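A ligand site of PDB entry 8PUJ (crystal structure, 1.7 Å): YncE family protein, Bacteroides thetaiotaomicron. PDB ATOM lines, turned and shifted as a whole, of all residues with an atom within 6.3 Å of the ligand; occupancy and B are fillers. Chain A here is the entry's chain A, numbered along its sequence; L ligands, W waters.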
ATOM      1  N   GLU A  11     -28.994 -31.549   9.555  1.00  0.00           N
ATOM      2  CA  GLU A  11     -28.614 -31.452   8.157  1.00  0.00           C
ATOM      3  C   GLU A  11     -27.421 -32.341   7.818  1.00  0.00           C
ATOM      4  O   GLU A  11     -27.237 -32.676   6.649  1.00  0.00           O
ATOM      5  CB  GLU A  11     -28.341 -29.978   7.791  1.00  0.00           C
ATOM      6  CG  GLU A  11     -29.592 -29.148   8.022  1.00  0.00           C
ATOM      7  CD  GLU A  11     -29.442 -27.703   7.554  1.00  0.00           C
ATOM      8  OE1 GLU A  11     -28.329 -27.307   7.180  1.00  0.00           O
ATOM      9  OE2 GLU A  11     -30.439 -26.961   7.609  1.00  0.00           O
ATOM     10  N   GLY A  12     -26.598 -32.729   8.808  1.00  0.00           N
ATOM     11  CA  GLY A  12     -25.364 -33.430   8.479  1.00  0.00           C
ATOM     12  C   GLY A  12     -24.398 -32.446   7.833  1.00  0.00           C
ATOM     13  O   GLY A  12     -24.636 -31.234   7.769  1.00  0.00           O
ATOM     14  N   ASN A  13     -23.296 -32.976   7.337  1.00  0.00           N
ATOM     15  CA  ASN A  13     -22.337 -32.126   6.647  1.00  0.00           C
ATOM     16  C   ASN A  13     -22.647 -32.185   5.152  1.00  0.00           C
ATOM     17  O   ASN A  13     -22.893 -33.271   4.604  1.00  0.00           O
ATOM     18  CB  ASN A  13     -20.930 -32.586   6.942  1.00  0.00           C
ATOM     19  CG  ASN A  13     -20.608 -32.531   8.418  1.00  0.00           C
ATOM     20  OD1 ASN A  13     -20.500 -33.551   9.068  1.00  0.00           O
ATOM     21  ND2 ASN A  13     -20.477 -31.317   8.941  1.00  0.00           N
ATOM     22  N   PHE A  14     -22.680 -31.012   4.527  1.00  0.00           N
ATOM     23  CA  PHE A  14     -23.044 -30.926   3.116  1.00  0.00           C
ATOM     24  C   PHE A  14     -22.132 -31.829   2.285  1.00  0.00           C
ATOM     25  O   PHE A  14     -20.906 -31.734   2.353  1.00  0.00           O
ATOM     26  CB  PHE A  14     -22.963 -29.458   2.667  1.00  0.00           C
ATOM     27  CG  PHE A  14     -23.330 -29.233   1.237  1.00  0.00           C
ATOM     28  CD1 PHE A  14     -24.387 -29.906   0.650  1.00  0.00           C
ATOM     29  CD2 PHE A  14     -22.607 -28.315   0.471  1.00  0.00           C
ATOM     30  CE1 PHE A  14     -24.719 -29.701  -0.681  1.00  0.00           C
ATOM     31  CE2 PHE A  14     -22.939 -28.088  -0.849  1.00  0.00           C
ATOM     32  CZ  PHE A  14     -23.993 -28.785  -1.433  1.00  0.00           C
ATOM     33  N   VAL A  47     -28.360 -33.311   3.825  1.00  0.00           N
ATOM     34  CA  VAL A  47     -29.025 -32.046   4.093  1.00  0.00           C
ATOM     35  C   VAL A  47     -30.520 -32.251   4.271  1.00  0.00           C
ATOM     36  O   VAL A  47     -31.345 -31.739   3.502  1.00  0.00           O
ATOM     37  CB  VAL A  47     -28.719 -30.977   3.029  1.00  0.00           C
ATOM     38  CG1 VAL A  47     -29.177 -29.601   3.536  1.00  0.00           C
ATOM     39  CG2 VAL A  47     -27.197 -30.923   2.708  1.00  0.00           C
ATOM     40  N   GLN A  49     -33.674 -30.905   5.497  1.00  0.00           N
ATOM     41  CA  GLN A  49     -33.844 -29.466   5.473  1.00  0.00           C
ATOM     42  C   GLN A  49     -35.106 -28.995   6.200  1.00  0.00           C
ATOM     43  O   GLN A  49     -35.093 -27.946   6.881  1.00  0.00           O
ATOM     44  CB  GLN A  49     -33.854 -28.966   3.992  1.00  0.00           C
ATOM     45  CG  GLN A  49     -34.311 -27.513   3.785  1.00  0.00           C
ATOM     46  CD  GLN A  49     -33.272 -26.521   4.228  1.00  0.00           C
ATOM     47  OE1 GLN A  49     -32.076 -26.792   4.178  1.00  0.00           O
ATOM     48  NE2 GLN A  49     -33.717 -25.337   4.668  1.00  0.00           N
ATOM     49  N   ASN A  63     -32.848 -32.271   1.179  1.00  0.00           N
ATOM     50  CA  ASN A  63     -32.528 -31.368   0.081  1.00  0.00           C
ATOM     51  C   ASN A  63     -31.529 -31.972  -0.884  1.00  0.00           C
ATOM     52  O   ASN A  63     -31.726 -31.970  -2.098  1.00  0.00           O
ATOM     53  CB  ASN A  63     -32.002 -30.059   0.659  1.00  0.00           C
ATOM     54  CG  ASN A  63     -31.258 -29.245  -0.359  1.00  0.00           C
ATOM     55  OD1 ASN A  63     -30.006 -29.250  -0.380  1.00  0.00           O
ATOM     56  ND2 ASN A  63     -31.991 -28.555  -1.240  1.00  0.00           N
ATOM     57  N   ASN A  64     -30.424 -32.474  -0.375  1.00  0.00           N
ATOM     58  CA  ASN A  64     -29.395 -32.905  -1.301  1.00  0.00           C
ATOM     59  C   ASN A  64     -29.486 -34.399  -1.605  1.00  0.00           C
ATOM     60  O   ASN A  64     -28.577 -34.965  -2.226  1.00  0.00           O
ATOM     61  CB  ASN A  64     -28.006 -32.509  -0.794  1.00  0.00           C
ATOM     62  CG  ASN A  64     -26.985 -32.492  -1.908  1.00  0.00           C
ATOM     63  OD1 ASN A  64     -27.318 -32.132  -3.056  1.00  0.00           O
ATOM     64  ND2 ASN A  64     -25.750 -32.898  -1.609  1.00  0.00           N
ATOM     65  N   SER A  87     -33.687 -29.986  -5.965  1.00  0.00           N
ATOM     66  CA  SER A  87     -32.959 -29.733  -4.720  1.00  0.00           C
ATOM     67  C   SER A  87     -34.010 -29.140  -3.760  1.00  0.00           C
ATOM     68  O   SER A  87     -34.064 -27.914  -3.561  1.00  0.00           O
ATOM     69  CB  SER A  87     -31.801 -28.765  -4.992  1.00  0.00           C
ATOM     70  OG  SER A  87     -30.855 -28.718  -3.935  1.00  0.00           O
ATOM     71  N   ARG A  89     -36.727 -27.828  -0.915  1.00  0.00           N
ATOM     72  CA  ARG A  89     -36.506 -26.977   0.243  1.00  0.00           C
ATOM     73  C   ARG A  89     -37.636 -27.146   1.243  1.00  0.00           C
ATOM     74  O   ARG A  89     -37.403 -27.641   2.352  1.00  0.00           O
ATOM     75  CB  ARG A  89     -36.368 -25.506  -0.196  1.00  0.00           C
ATOM     76  CG  ARG A  89     -35.256 -25.315  -1.247  1.00  0.00           C
ATOM     77  CD  ARG A  89     -33.890 -25.691  -0.670  1.00  0.00           C
ATOM     78  NE  ARG A  89     -33.445 -24.701   0.309  1.00  0.00           N
ATOM     79  CZ  ARG A  89     -32.296 -24.759   0.955  1.00  0.00           C
ATOM     80  NH1 ARG A  89     -31.445 -25.770   0.773  1.00  0.00           N
ATOM     81  NH2 ARG A  89     -32.006 -23.801   1.838  1.00  0.00           N
ATOM     82  N   ILE A 104     -33.956 -25.108  -4.574  1.00  0.00           N
ATOM     83  CA  ILE A 104     -32.816 -24.282  -4.934  1.00  0.00           C
ATOM     84  C   ILE A 104     -32.211 -24.838  -6.229  1.00  0.00           C
ATOM     85  O   ILE A 104     -32.426 -26.017  -6.581  1.00  0.00           O
ATOM     86  CB  ILE A 104     -31.806 -24.206  -3.776  1.00  0.00           C
ATOM     87  CG1 ILE A 104     -30.716 -23.208  -4.079  1.00  0.00           C
ATOM     88  CG2 ILE A 104     -31.253 -25.589  -3.482  1.00  0.00           C
ATOM     89  CD1 ILE A 104     -29.796 -22.887  -2.842  1.00  0.00           C
ATOM     90  N   TRP A 105     -31.556 -23.961  -6.987  1.00  0.00           N
ATOM     91  CA  TRP A 105     -30.967 -24.332  -8.282  1.00  0.00           C
ATOM     92  C   TRP A 105     -32.028 -24.764  -9.280  1.00  0.00           C
ATOM     93  O   TRP A 105     -31.793 -25.617 -10.143  1.00  0.00           O
ATOM     94  CB  TRP A 105     -29.893 -25.443  -8.143  1.00  0.00           C
ATOM     95  CG  TRP A 105     -28.985 -25.192  -6.974  1.00  0.00           C
ATOM     96  CD1 TRP A 105     -28.742 -26.045  -5.911  1.00  0.00           C
ATOM     97  CD2 TRP A 105     -28.217 -24.021  -6.733  1.00  0.00           C
ATOM     98  NE1 TRP A 105     -27.871 -25.453  -5.018  1.00  0.00           N
ATOM     99  CE2 TRP A 105     -27.541 -24.214  -5.498  1.00  0.00           C
ATOM    100  CE3 TRP A 105     -28.040 -22.820  -7.421  1.00  0.00           C
ATOM    101  CZ2 TRP A 105     -26.700 -23.245  -4.956  1.00  0.00           C
ATOM    102  CZ3 TRP A 105     -27.190 -21.869  -6.892  1.00  0.00           C
ATOM    103  CH2 TRP A 105     -26.533 -22.089  -5.658  1.00  0.00           C
ATOM    104  N   GLU A 136     -38.148 -20.788  -1.427  1.00  0.00           N
ATOM    105  CA  GLU A 136     -37.844 -21.240  -0.083  1.00  0.00           C
ATOM    106  C   GLU A 136     -39.116 -21.482   0.729  1.00  0.00           C
ATOM    107  O   GLU A 136     -39.850 -22.447   0.429  1.00  0.00           O
ATOM    108  CB  GLU A 136     -36.902 -20.202   0.581  1.00  0.00           C
ATOM    109  CG  GLU A 136     -36.186 -20.717   1.814  1.00  0.00           C
ATOM    110  CD  GLU A 136     -35.078 -21.752   1.607  1.00  0.00           C
ATOM    111  OE1 GLU A 136     -34.391 -21.999   2.653  1.00  0.00           O
ATOM    112  OE2 GLU A 136     -34.720 -22.087   0.429  1.00  0.00           O
ATOM    113  N   TRP A 150     -34.643 -16.981  -1.872  1.00  0.00           N
ATOM    114  CA  TRP A 150     -33.533 -16.725  -0.953  1.00  0.00           C
ATOM    115  C   TRP A 150     -32.171 -16.553  -1.651  1.00  0.00           C
ATOM    116  O   TRP A 150     -31.649 -15.429  -1.761  1.00  0.00           O
ATOM    117  CB  TRP A 150     -33.485 -17.843   0.098  1.00  0.00           C
ATOM    118  CG  TRP A 150     -32.222 -17.762   0.936  1.00  0.00           C
ATOM    119  CD1 TRP A 150     -31.773 -16.687   1.672  1.00  0.00           C
ATOM    120  CD2 TRP A 150     -31.239 -18.797   1.073  1.00  0.00           C
ATOM    121  NE1 TRP A 150     -30.541 -16.999   2.232  1.00  0.00           N
ATOM    122  CE2 TRP A 150     -30.218 -18.292   1.894  1.00  0.00           C
ATOM    123  CE3 TRP A 150     -31.142 -20.097   0.564  1.00  0.00           C
ATOM    124  CZ2 TRP A 150     -29.079 -19.062   2.222  1.00  0.00           C
ATOM    125  CZ3 TRP A 150     -30.018 -20.861   0.896  1.00  0.00           C
ATOM    126  CH2 TRP A 150     -29.003 -20.329   1.701  1.00  0.00           C
ATOM    127  N   SER A 151     -31.574 -17.641  -2.100  1.00  0.00           N
ATOM    128  CA  SER A 151     -30.195 -17.630  -2.566  1.00  0.00           C
ATOM    129  C   SER A 151     -30.105 -16.899  -3.910  1.00  0.00           C
ATOM    130  O   SER A 151     -30.767 -17.307  -4.882  1.00  0.00           O
ATOM    131  CB  SER A 151     -29.716 -19.089  -2.711  1.00  0.00           C
ATOM    132  OG  SER A 151     -28.472 -19.083  -3.354  1.00  0.00           O
ATOM    133  N   TYR A 152     -29.309 -15.809  -3.954  1.00  0.00           N
ATOM    134  CA  TYR A 152     -29.148 -14.995  -5.166  1.00  0.00           C
ATOM    135  C   TYR A 152     -30.481 -14.419  -5.647  1.00  0.00           C
ATOM    136  O   TYR A 152     -30.668 -14.160  -6.861  1.00  0.00           O
ATOM    137  CB  TYR A 152     -28.496 -15.793  -6.295  1.00  0.00           C
ATOM    138  CG  TYR A 152     -27.175 -16.458  -5.871  1.00  0.00           C
ATOM    139  CD1 TYR A 152     -26.376 -15.881  -4.869  1.00  0.00           C
ATOM    140  CD2 TYR A 152     -26.780 -17.674  -6.409  1.00  0.00           C
ATOM    141  CE1 TYR A 152     -25.150 -16.504  -4.453  1.00  0.00           C
ATOM    142  CE2 TYR A 152     -25.571 -18.293  -6.011  1.00  0.00           C
ATOM    143  CZ  TYR A 152     -24.769 -17.692  -5.056  1.00  0.00           C
ATOM    144  OH  TYR A 152     -23.581 -18.314  -4.661  1.00  0.00           O
ATOM    145  N   GLN A 175     -31.845 -11.604  -0.416  1.00  0.00           N
ATOM    146  CA  GLN A 175     -31.848 -12.904   0.260  1.00  0.00           C
ATOM    147  C   GLN A 175     -32.762 -12.922   1.490  1.00  0.00           C
ATOM    148  O   GLN A 175     -32.323 -13.273   2.586  1.00  0.00           O
ATOM    149  CB  GLN A 175     -30.426 -13.320   0.604  1.00  0.00           C
ATOM    150  CG  GLN A 175     -29.552 -13.226  -0.677  1.00  0.00           C
ATOM    151  CD  GLN A 175     -28.314 -14.119  -0.644  1.00  0.00           C
ATOM    152  OE1 GLN A 175     -27.749 -14.448  -1.713  1.00  0.00           O
ATOM    153  NE2 GLN A 175     -27.847 -14.456   0.567  1.00  0.00           N
ATOM    154  N   ASP A 192     -30.861 -11.898   4.962  1.00  0.00           N
ATOM    155  CA  ASP A 192     -29.527 -12.176   5.572  1.00  0.00           C
ATOM    156  C   ASP A 192     -28.468 -11.155   5.111  1.00  0.00           C
ATOM    157  O   ASP A 192     -27.374 -11.179   5.658  1.00  0.00           O
ATOM    158  CB  ASP A 192     -29.076 -13.618   5.378  1.00  0.00           C
ATOM    159  CG  ASP A 192     -28.800 -14.076   3.960  1.00  0.00           C
ATOM    160  OD1 ASP A 192     -28.545 -13.234   3.101  1.00  0.00           O
ATOM    161  OD2 ASP A 192     -28.828 -15.307   3.734  1.00  0.00           O
ATOM    162  N   GLY A 194     -26.864 -11.021   2.329  1.00  0.00           N
ATOM    163  CA  GLY A 194     -25.742 -11.487   1.523  1.00  0.00           C
ATOM    164  C   GLY A 194     -24.533 -11.616   2.430  1.00  0.00           C
ATOM    165  O   GLY A 194     -24.640 -11.898   3.617  1.00  0.00           O
ATOM    166  N   TYR A 195     -23.344 -11.425   1.848  1.00  0.00           N
ATOM    167  CA  TYR A 195     -22.124 -11.490   2.676  1.00  0.00           C
ATOM    168  C   TYR A 195     -21.028 -10.788   1.898  1.00  0.00           C
ATOM    169  O   TYR A 195     -21.135 -10.585   0.686  1.00  0.00           O
ATOM    170  CB  TYR A 195     -21.760 -12.922   3.003  1.00  0.00           C
ATOM    171  CG  TYR A 195     -21.481 -13.815   1.800  1.00  0.00           C
ATOM    172  CD1 TYR A 195     -20.212 -13.928   1.262  1.00  0.00           C
ATOM    173  CD2 TYR A 195     -22.491 -14.584   1.229  1.00  0.00           C
ATOM    174  CE1 TYR A 195     -19.954 -14.741   0.195  1.00  0.00           C
ATOM    175  CE2 TYR A 195     -22.251 -15.407   0.165  1.00  0.00           C
ATOM    176  CZ  TYR A 195     -20.973 -15.493  -0.363  1.00  0.00           C
ATOM    177  OH  TYR A 195     -20.732 -16.315  -1.427  1.00  0.00           O
ATOM    178  N   SER A 198     -19.781 -11.831  -1.556  1.00  0.00           N
ATOM    179  CA  SER A 198     -20.758 -12.592  -2.310  1.00  0.00           C
ATOM    180  C   SER A 198     -20.712 -12.227  -3.798  1.00  0.00           C
ATOM    181  O   SER A 198     -20.576 -11.048  -4.136  1.00  0.00           O
ATOM    182  CB  SER A 198     -22.147 -12.294  -1.748  1.00  0.00           C
ATOM    183  OG  SER A 198     -23.168 -12.728  -2.608  1.00  0.00           O
ATOM    184  N   PRO A 199     -20.894 -13.193  -4.699  1.00  0.00           N
ATOM    185  CA  PRO A 199     -21.083 -12.850  -6.110  1.00  0.00           C
ATOM    186  C   PRO A 199     -22.395 -12.111  -6.375  1.00  0.00           C
ATOM    187  O   PRO A 199     -22.573 -11.571  -7.474  1.00  0.00           O
ATOM    188  CB  PRO A 199     -21.082 -14.221  -6.809  1.00  0.00           C
ATOM    189  CG  PRO A 199     -21.582 -15.182  -5.741  1.00  0.00           C
ATOM    190  CD  PRO A 199     -20.993 -14.650  -4.458  1.00  0.00           C
ATOM    191  N   TYR A 272     -28.676 -21.947  14.945  1.00  0.00           N
ATOM    192  CA  TYR A 272     -28.949 -22.229  13.534  1.00  0.00           C
ATOM    193  C   TYR A 272     -30.407 -22.528  13.237  1.00  0.00           C
ATOM    194  O   TYR A 272     -30.826 -22.358  12.081  1.00  0.00           O
ATOM    195  CB  TYR A 272     -28.064 -23.392  13.059  1.00  0.00           C
ATOM    196  CG  TYR A 272     -28.040 -23.578  11.578  1.00  0.00           C
ATOM    197  CD1 TYR A 272     -27.596 -22.562  10.723  1.00  0.00           C
ATOM    198  CD2 TYR A 272     -28.441 -24.779  11.014  1.00  0.00           C
ATOM    199  CE1 TYR A 272     -27.550 -22.766   9.336  1.00  0.00           C
ATOM    200  CE2 TYR A 272     -28.397 -24.978   9.636  1.00  0.00           C
ATOM    201  CZ  TYR A 272     -27.955 -23.972   8.809  1.00  0.00           C
ATOM    202  OH  TYR A 272     -27.921 -24.191   7.452  1.00  0.00           O
ATOM    203  N   ASP A 290     -20.095 -25.601  15.925  1.00  0.00           N
ATOM    204  CA  ASP A 290     -19.056 -25.190  14.982  1.00  0.00           C
ATOM    205  C   ASP A 290     -19.314 -25.766  13.595  1.00  0.00           C
ATOM    206  O   ASP A 290     -18.419 -25.723  12.742  1.00  0.00           O
ATOM    207  CB  ASP A 290     -17.667 -25.577  15.500  1.00  0.00           C
ATOM    208  CG  ASP A 290     -17.533 -27.071  15.742  1.00  0.00           C
ATOM    209  OD1 ASP A 290     -18.495 -27.813  15.527  1.00  0.00           O
ATOM    210  OD2 ASP A 290     -16.452 -27.509  16.165  1.00  0.00           O
ATOM    211  N   TYR A 291     -20.494 -26.341  13.370  1.00  0.00           N
ATOM    212  CA  TYR A 291     -20.898 -27.034  12.156  1.00  0.00           C
ATOM    213  C   TYR A 291     -20.126 -28.331  11.939  1.00  0.00           C
ATOM    214  O   TYR A 291     -20.125 -28.841  10.816  1.00  0.00           O
ATOM    215  CB  TYR A 291     -20.717 -26.184  10.895  1.00  0.00           C
ATOM    216  CG  TYR A 291     -21.387 -24.820  10.910  1.00  0.00           C
ATOM    217  CD1 TYR A 291     -22.763 -24.722  10.947  1.00  0.00           C
ATOM    218  CD2 TYR A 291     -20.630 -23.651  10.838  1.00  0.00           C
ATOM    219  CE1 TYR A 291     -23.391 -23.474  10.932  1.00  0.00           C
ATOM    220  CE2 TYR A 291     -21.233 -22.410  10.808  1.00  0.00           C
ATOM    221  CZ  TYR A 291     -22.610 -22.329  10.842  1.00  0.00           C
ATOM    222  OH  TYR A 291     -23.211 -21.107  10.823  1.00  0.00           O
ATOM    223  N   GLN A 292     -19.444 -28.849  12.958  1.00  0.00           N
ATOM    224  CA  GLN A 292     -18.678 -30.088  12.790  1.00  0.00           C
ATOM    225  C   GLN A 292     -19.034 -31.116  13.844  1.00  0.00           C
ATOM    226  O   GLN A 292     -19.320 -32.268  13.521  1.00  0.00           O
ATOM    227  CB  GLN A 292     -17.177 -29.791  12.842  1.00  0.00           C
ATOM    228  CG  GLN A 292     -16.659 -28.940  11.675  1.00  0.00           C
ATOM    229  CD  GLN A 292     -16.065 -29.779  10.544  1.00  0.00           C
ATOM    230  OE1 GLN A 292     -14.973 -30.331  10.672  1.00  0.00           O
ATOM    231  NE2 GLN A 292     -16.797 -29.863   9.426  1.00  0.00           N
ATOM    232  N   ILE A 315     -25.314 -30.488  12.713  1.00  0.00           N
ATOM    233  CA  ILE A 315     -25.982 -29.288  12.205  1.00  0.00           C
ATOM    234  C   ILE A 315     -27.503 -29.440  12.324  1.00  0.00           C
ATOM    235  O   ILE A 315     -28.230 -29.471  11.317  1.00  0.00           O
ATOM    236  CB  ILE A 315     -25.538 -28.951  10.770  1.00  0.00           C
ATOM    237  CG1 ILE A 315     -24.007 -28.863  10.710  1.00  0.00           C
ATOM    238  CG2 ILE A 315     -26.099 -27.576  10.270  1.00  0.00           C
ATOM    239  CD1 ILE A 315     -23.482 -28.394   9.348  1.00  0.00           C
HETATM  240  N1  LIG L   1     -19.208 -24.469   7.738  1.00  0.00           N
HETATM  241  C1  LIG L   1     -19.990 -25.272   7.037  1.00  0.00           C
HETATM  242  O1  LIG L   1     -19.852 -26.486   7.035  1.00  0.00           O
HETATM  243  C2  LIG L   1     -21.085 -24.583   6.266  1.00  0.00           C
HETATM  244  C3  LIG L   1     -22.117 -24.019   7.245  1.00  0.00           C
HETATM  245  C4  LIG L   1     -23.333 -23.412   6.516  1.00  0.00           C
HETATM  246  C5  LIG L   1     -24.367 -22.877   7.534  1.00  0.00           C
HETATM  247  C6  LIG L   1     -23.957 -24.463   5.602  1.00  0.00           C
HETATM  248  C7  LIG L   1     -24.545 -23.613   4.467  1.00  0.00           C
HETATM  249  C8  LIG L   1     -24.953 -25.402   6.321  1.00  0.00           C
HETATM  250  C9  LIG L   1     -24.662 -26.854   6.006  1.00  0.00           C
HETATM  251  N2  LIG L   1     -25.624 -27.780   6.169  1.00  0.00           N
HETATM  252  O2  LIG L   1     -23.554 -27.188   5.566  1.00  0.00           O
HETATM  253  C10 LIG L   1     -22.944 -22.314   5.511  1.00  0.00           C
HETATM  254  N3  LIG L   1     -23.407 -22.702   4.234  1.00  0.00           N
HETATM  255  C11 LIG L   1     -22.244 -21.193   5.707  1.00  0.00           C
HETATM  256  C12 LIG L   1     -21.698 -20.735   7.045  1.00  0.00           C
HETATM  257  C13 LIG L   1     -21.967 -20.322   4.583  1.00  0.00           C
HETATM  258  C14 LIG L   1     -20.746 -19.474   4.540  1.00  0.00           C
HETATM  259  C15 LIG L   1     -19.555 -20.291   4.046  1.00  0.00           C
HETATM  260  C16 LIG L   1     -19.099 -21.288   5.094  1.00  0.00           C
HETATM  261  C17 LIG L   1     -18.134 -20.695   6.099  1.00  0.00           C
HETATM  262  N4  LIG L   1     -18.015 -19.365   6.197  1.00  0.00           N
HETATM  263  O3  LIG L   1     -17.496 -21.454   6.812  1.00  0.00           O
HETATM  264  C18 LIG L   1     -21.145 -18.429   3.525  1.00  0.00           C
HETATM  265  C19 LIG L   1     -20.032 -17.984   2.578  1.00  0.00           C
HETATM  266  C20 LIG L   1     -21.822 -17.270   4.254  1.00  0.00           C
HETATM  267  C21 LIG L   1     -22.171 -19.176   2.719  1.00  0.00           C
HETATM  268  N5  LIG L   1     -22.882 -20.070   3.508  1.00  0.00           N
HETATM  269  C22 LIG L   1     -22.371 -18.829   1.443  1.00  0.00           C
HETATM  270  C23 LIG L   1     -23.240 -19.652   0.596  1.00  0.00           C
HETATM  271  C24 LIG L   1     -23.606 -19.284  -0.808  1.00  0.00           C
HETATM  272  C25 LIG L   1     -22.617 -19.896  -1.794  1.00  0.00           C
HETATM  273  C26 LIG L   1     -21.183 -19.981  -1.246  1.00  0.00           C
HETATM  274  C27 LIG L   1     -20.181 -20.149  -2.367  1.00  0.00           C
HETATM  275  N6  LIG L   1     -20.652 -20.047  -3.613  1.00  0.00           N
HETATM  276  O4  LIG L   1     -18.999 -20.355  -2.108  1.00  0.00           O
HETATM  277  C28 LIG L   1     -24.992 -19.954  -0.968  1.00  0.00           C
HETATM  278  C29 LIG L   1     -25.161 -20.451  -2.390  1.00  0.00           C
HETATM  279  C30 LIG L   1     -26.106 -18.940  -0.727  1.00  0.00           C
HETATM  280  C31 LIG L   1     -25.821 -17.873   0.280  1.00  0.00           C
HETATM  281  N7  LIG L   1     -25.939 -18.253   1.576  1.00  0.00           N
HETATM  282  O5  LIG L   1     -25.514 -16.728  -0.072  1.00  0.00           O
HETATM  283  C32 LIG L   1     -24.996 -21.032   0.131  1.00  0.00           C
HETATM  284  N8  LIG L   1     -23.824 -20.880   0.958  1.00  0.00           N
HETATM  285  C33 LIG L   1     -25.880 -22.053   0.281  1.00  0.00           C
HETATM  286  C34 LIG L   1     -27.116 -22.260  -0.564  1.00  0.00           C
HETATM  287  C35 LIG L   1     -25.667 -23.129   1.251  1.00  0.00           C
HETATM  288  C36 LIG L   1     -26.501 -24.378   1.363  1.00  0.00           C
HETATM  289  C37 LIG L   1     -26.194 -25.434   0.278  1.00  0.00           C
HETATM  290  C38 LIG L   1     -27.500 -26.083  -0.212  1.00  0.00           C
HETATM  291  C39 LIG L   1     -27.317 -26.710  -1.581  1.00  0.00           C
HETATM  292  N9  LIG L   1     -27.769 -27.960  -1.724  1.00  0.00           N
HETATM  293  O6  LIG L   1     -26.755 -26.098  -2.492  1.00  0.00           O
HETATM  294  C40 LIG L   1     -26.163 -24.851   2.783  1.00  0.00           C
HETATM  295  C41 LIG L   1     -26.111 -26.356   2.968  1.00  0.00           C
HETATM  296  C42 LIG L   1     -24.766 -24.234   3.079  1.00  0.00           C
HETATM  297  C43 LIG L   1     -23.634 -25.231   2.763  1.00  0.00           C
HETATM  298  N10 LIG L   1     -24.539 -23.177   2.073  1.00  0.00           N
HETATM  299 CO1  LIG L   1     -23.737 -21.592   2.722  1.00  0.00          CO
HETATM  300  C44 LIG L   1     -27.221 -24.305   3.744  1.00  0.00           C
HETATM  301  C45 LIG L   1     -28.599 -24.956   3.541  1.00  0.00           C
HETATM  302  O7  LIG L   1     -29.138 -25.724   4.345  1.00  0.00           O
HETATM  303  N11 LIG L   1     -29.230 -24.640   2.422  1.00  0.00           N
HETATM  304  C46 LIG L   1     -18.398 -24.995   8.823  1.00  0.00           C
HETATM  305  C47 LIG L   1     -17.025 -24.355   8.812  1.00  0.00           C
HETATM  306  C48 LIG L   1     -16.435 -24.775   7.485  1.00  0.00           C
HETATM  307  O8  LIG L   1     -17.125 -22.926   8.948  1.00  0.00           O
HETATM  308  O   HOH W   1     -30.941 -24.314   6.982  1.00  0.00           O
HETATM  309  O   HOH W   2     -21.479 -28.962   6.084  1.00  0.00           O
HETATM  310  O   HOH W   3     -25.068 -14.252  -1.390  1.00  0.00           O
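The guanidinium group (NH2) of Arg 89 lies close to a nitrogen (N11) of the ligand, at 3.0 Å. O of Gly 12 touches N2 of the ligand, 3.9 Å away. CE1 of Phe 14 touches N9 of the ligand (3.7 Å). Val 47 touches the ligand (CG1 to O7, 3.96 Å). Ser 87 touches the ligand. Ile 104 touches the ligand (CD1 to C34, 3.6 Å). Trp 150 touches the ligand. OG of Ser 151 touches C30 of the ligand (3.5 Å). Tyr 152 touches the ligand (OH to C25, 3.4 Å). Tyr 195 touches the ligand (CE2 to O5, 3.5 Å). Tyr 272 touches the ligand (OH to C8, 3.4 Å). O of Asp 290 touches C46 of the ligand, 3.99 Å away. Tyr 291 touches the ligand. Ile 315 touches the ligand (CD1 to C9, 3.9 Å). Hydrophobic or aromatic side chains that line the ligand: Phe 14, Val 47, Ile 104, Trp 105, Trp 150, Tyr 152, Tyr 195, Tyr 272, Tyr 291 and Ile 315. The nearest printed residue that does not touch the ligand is Asn 64 (4.4 Å).
N of Ile 104 is in hydrogen-bond range of O of Ser 87. ND2 of Asn 63 sits close to NH1 of Arg 89 (3.5 Å). The side-chain carboxylate of Asp 192 is in hydrogen-bond range of the side-chain amide nitrogen of Gln 175, at 2.9 Å. The indole nitrogen (NE1) of Trp 150 lies within hydrogen-bond range of the side-chain carboxylate (OD2) of Asp 192, at 2.8 Å. The side-chain hydroxyl (OH) of Tyr 272 sits at hydrogen-bond distance from the side-chain carboxylate (OE1) of Glu 11. The side-chain amide nitrogen (ND2) of Asn 13 lies within hydrogen-bond range of the backbone carbonyl oxygen (O) of Tyr 291, 3.1 Å away. OE1 of Gln 175 is in hydrogen-bond range of N of Tyr 152, 3.1 Å away. OE2 of Glu 136 is in salt-bridge range of NE of Arg 89, 2.9 Å away.
Water W2 lies within hydrogen-bond range of O2 of the ligand (2.8 Å) and N of Phe 14 (2.8 Å). Water W3 lies within hydrogen-bond range of the side-chain amide oxygen of Gln 175 (2.7 Å), the side-chain hydroxyl of Ser 198 (2.7 Å) and an oxygen (O5) of the ligand (2.8 Å). Water W1 lies within hydrogen-bond range of the side-chain carboxylate (OE2) of Glu 11 (2.8 Å), the side-chain hydroxyl (OH) of Tyr 272 (3.1 Å) and an oxygen (O7) of the ligand (3.5 Å).
The indole nitrogen (NE1) of Trp 105 is in hydrogen-bond range of an oxygen (O6) of the ligand (2.8 Å). A nitrogen (N2) of the ligand is in hydrogen-bond range of the side-chain carboxylate (OE1) of Glu 11, at 2.9 Å. OD1 of Asn 63 sits at hydrogen-bond distance from N9 of the ligand, at 2.9 Å. The side-chain amide nitrogen (NE2) of Gln 175 is in hydrogen-bond range of an oxygen (O5) of the ligand (3.3 Å). OE1 of Gln 49 sits close to O7 of the ligand.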
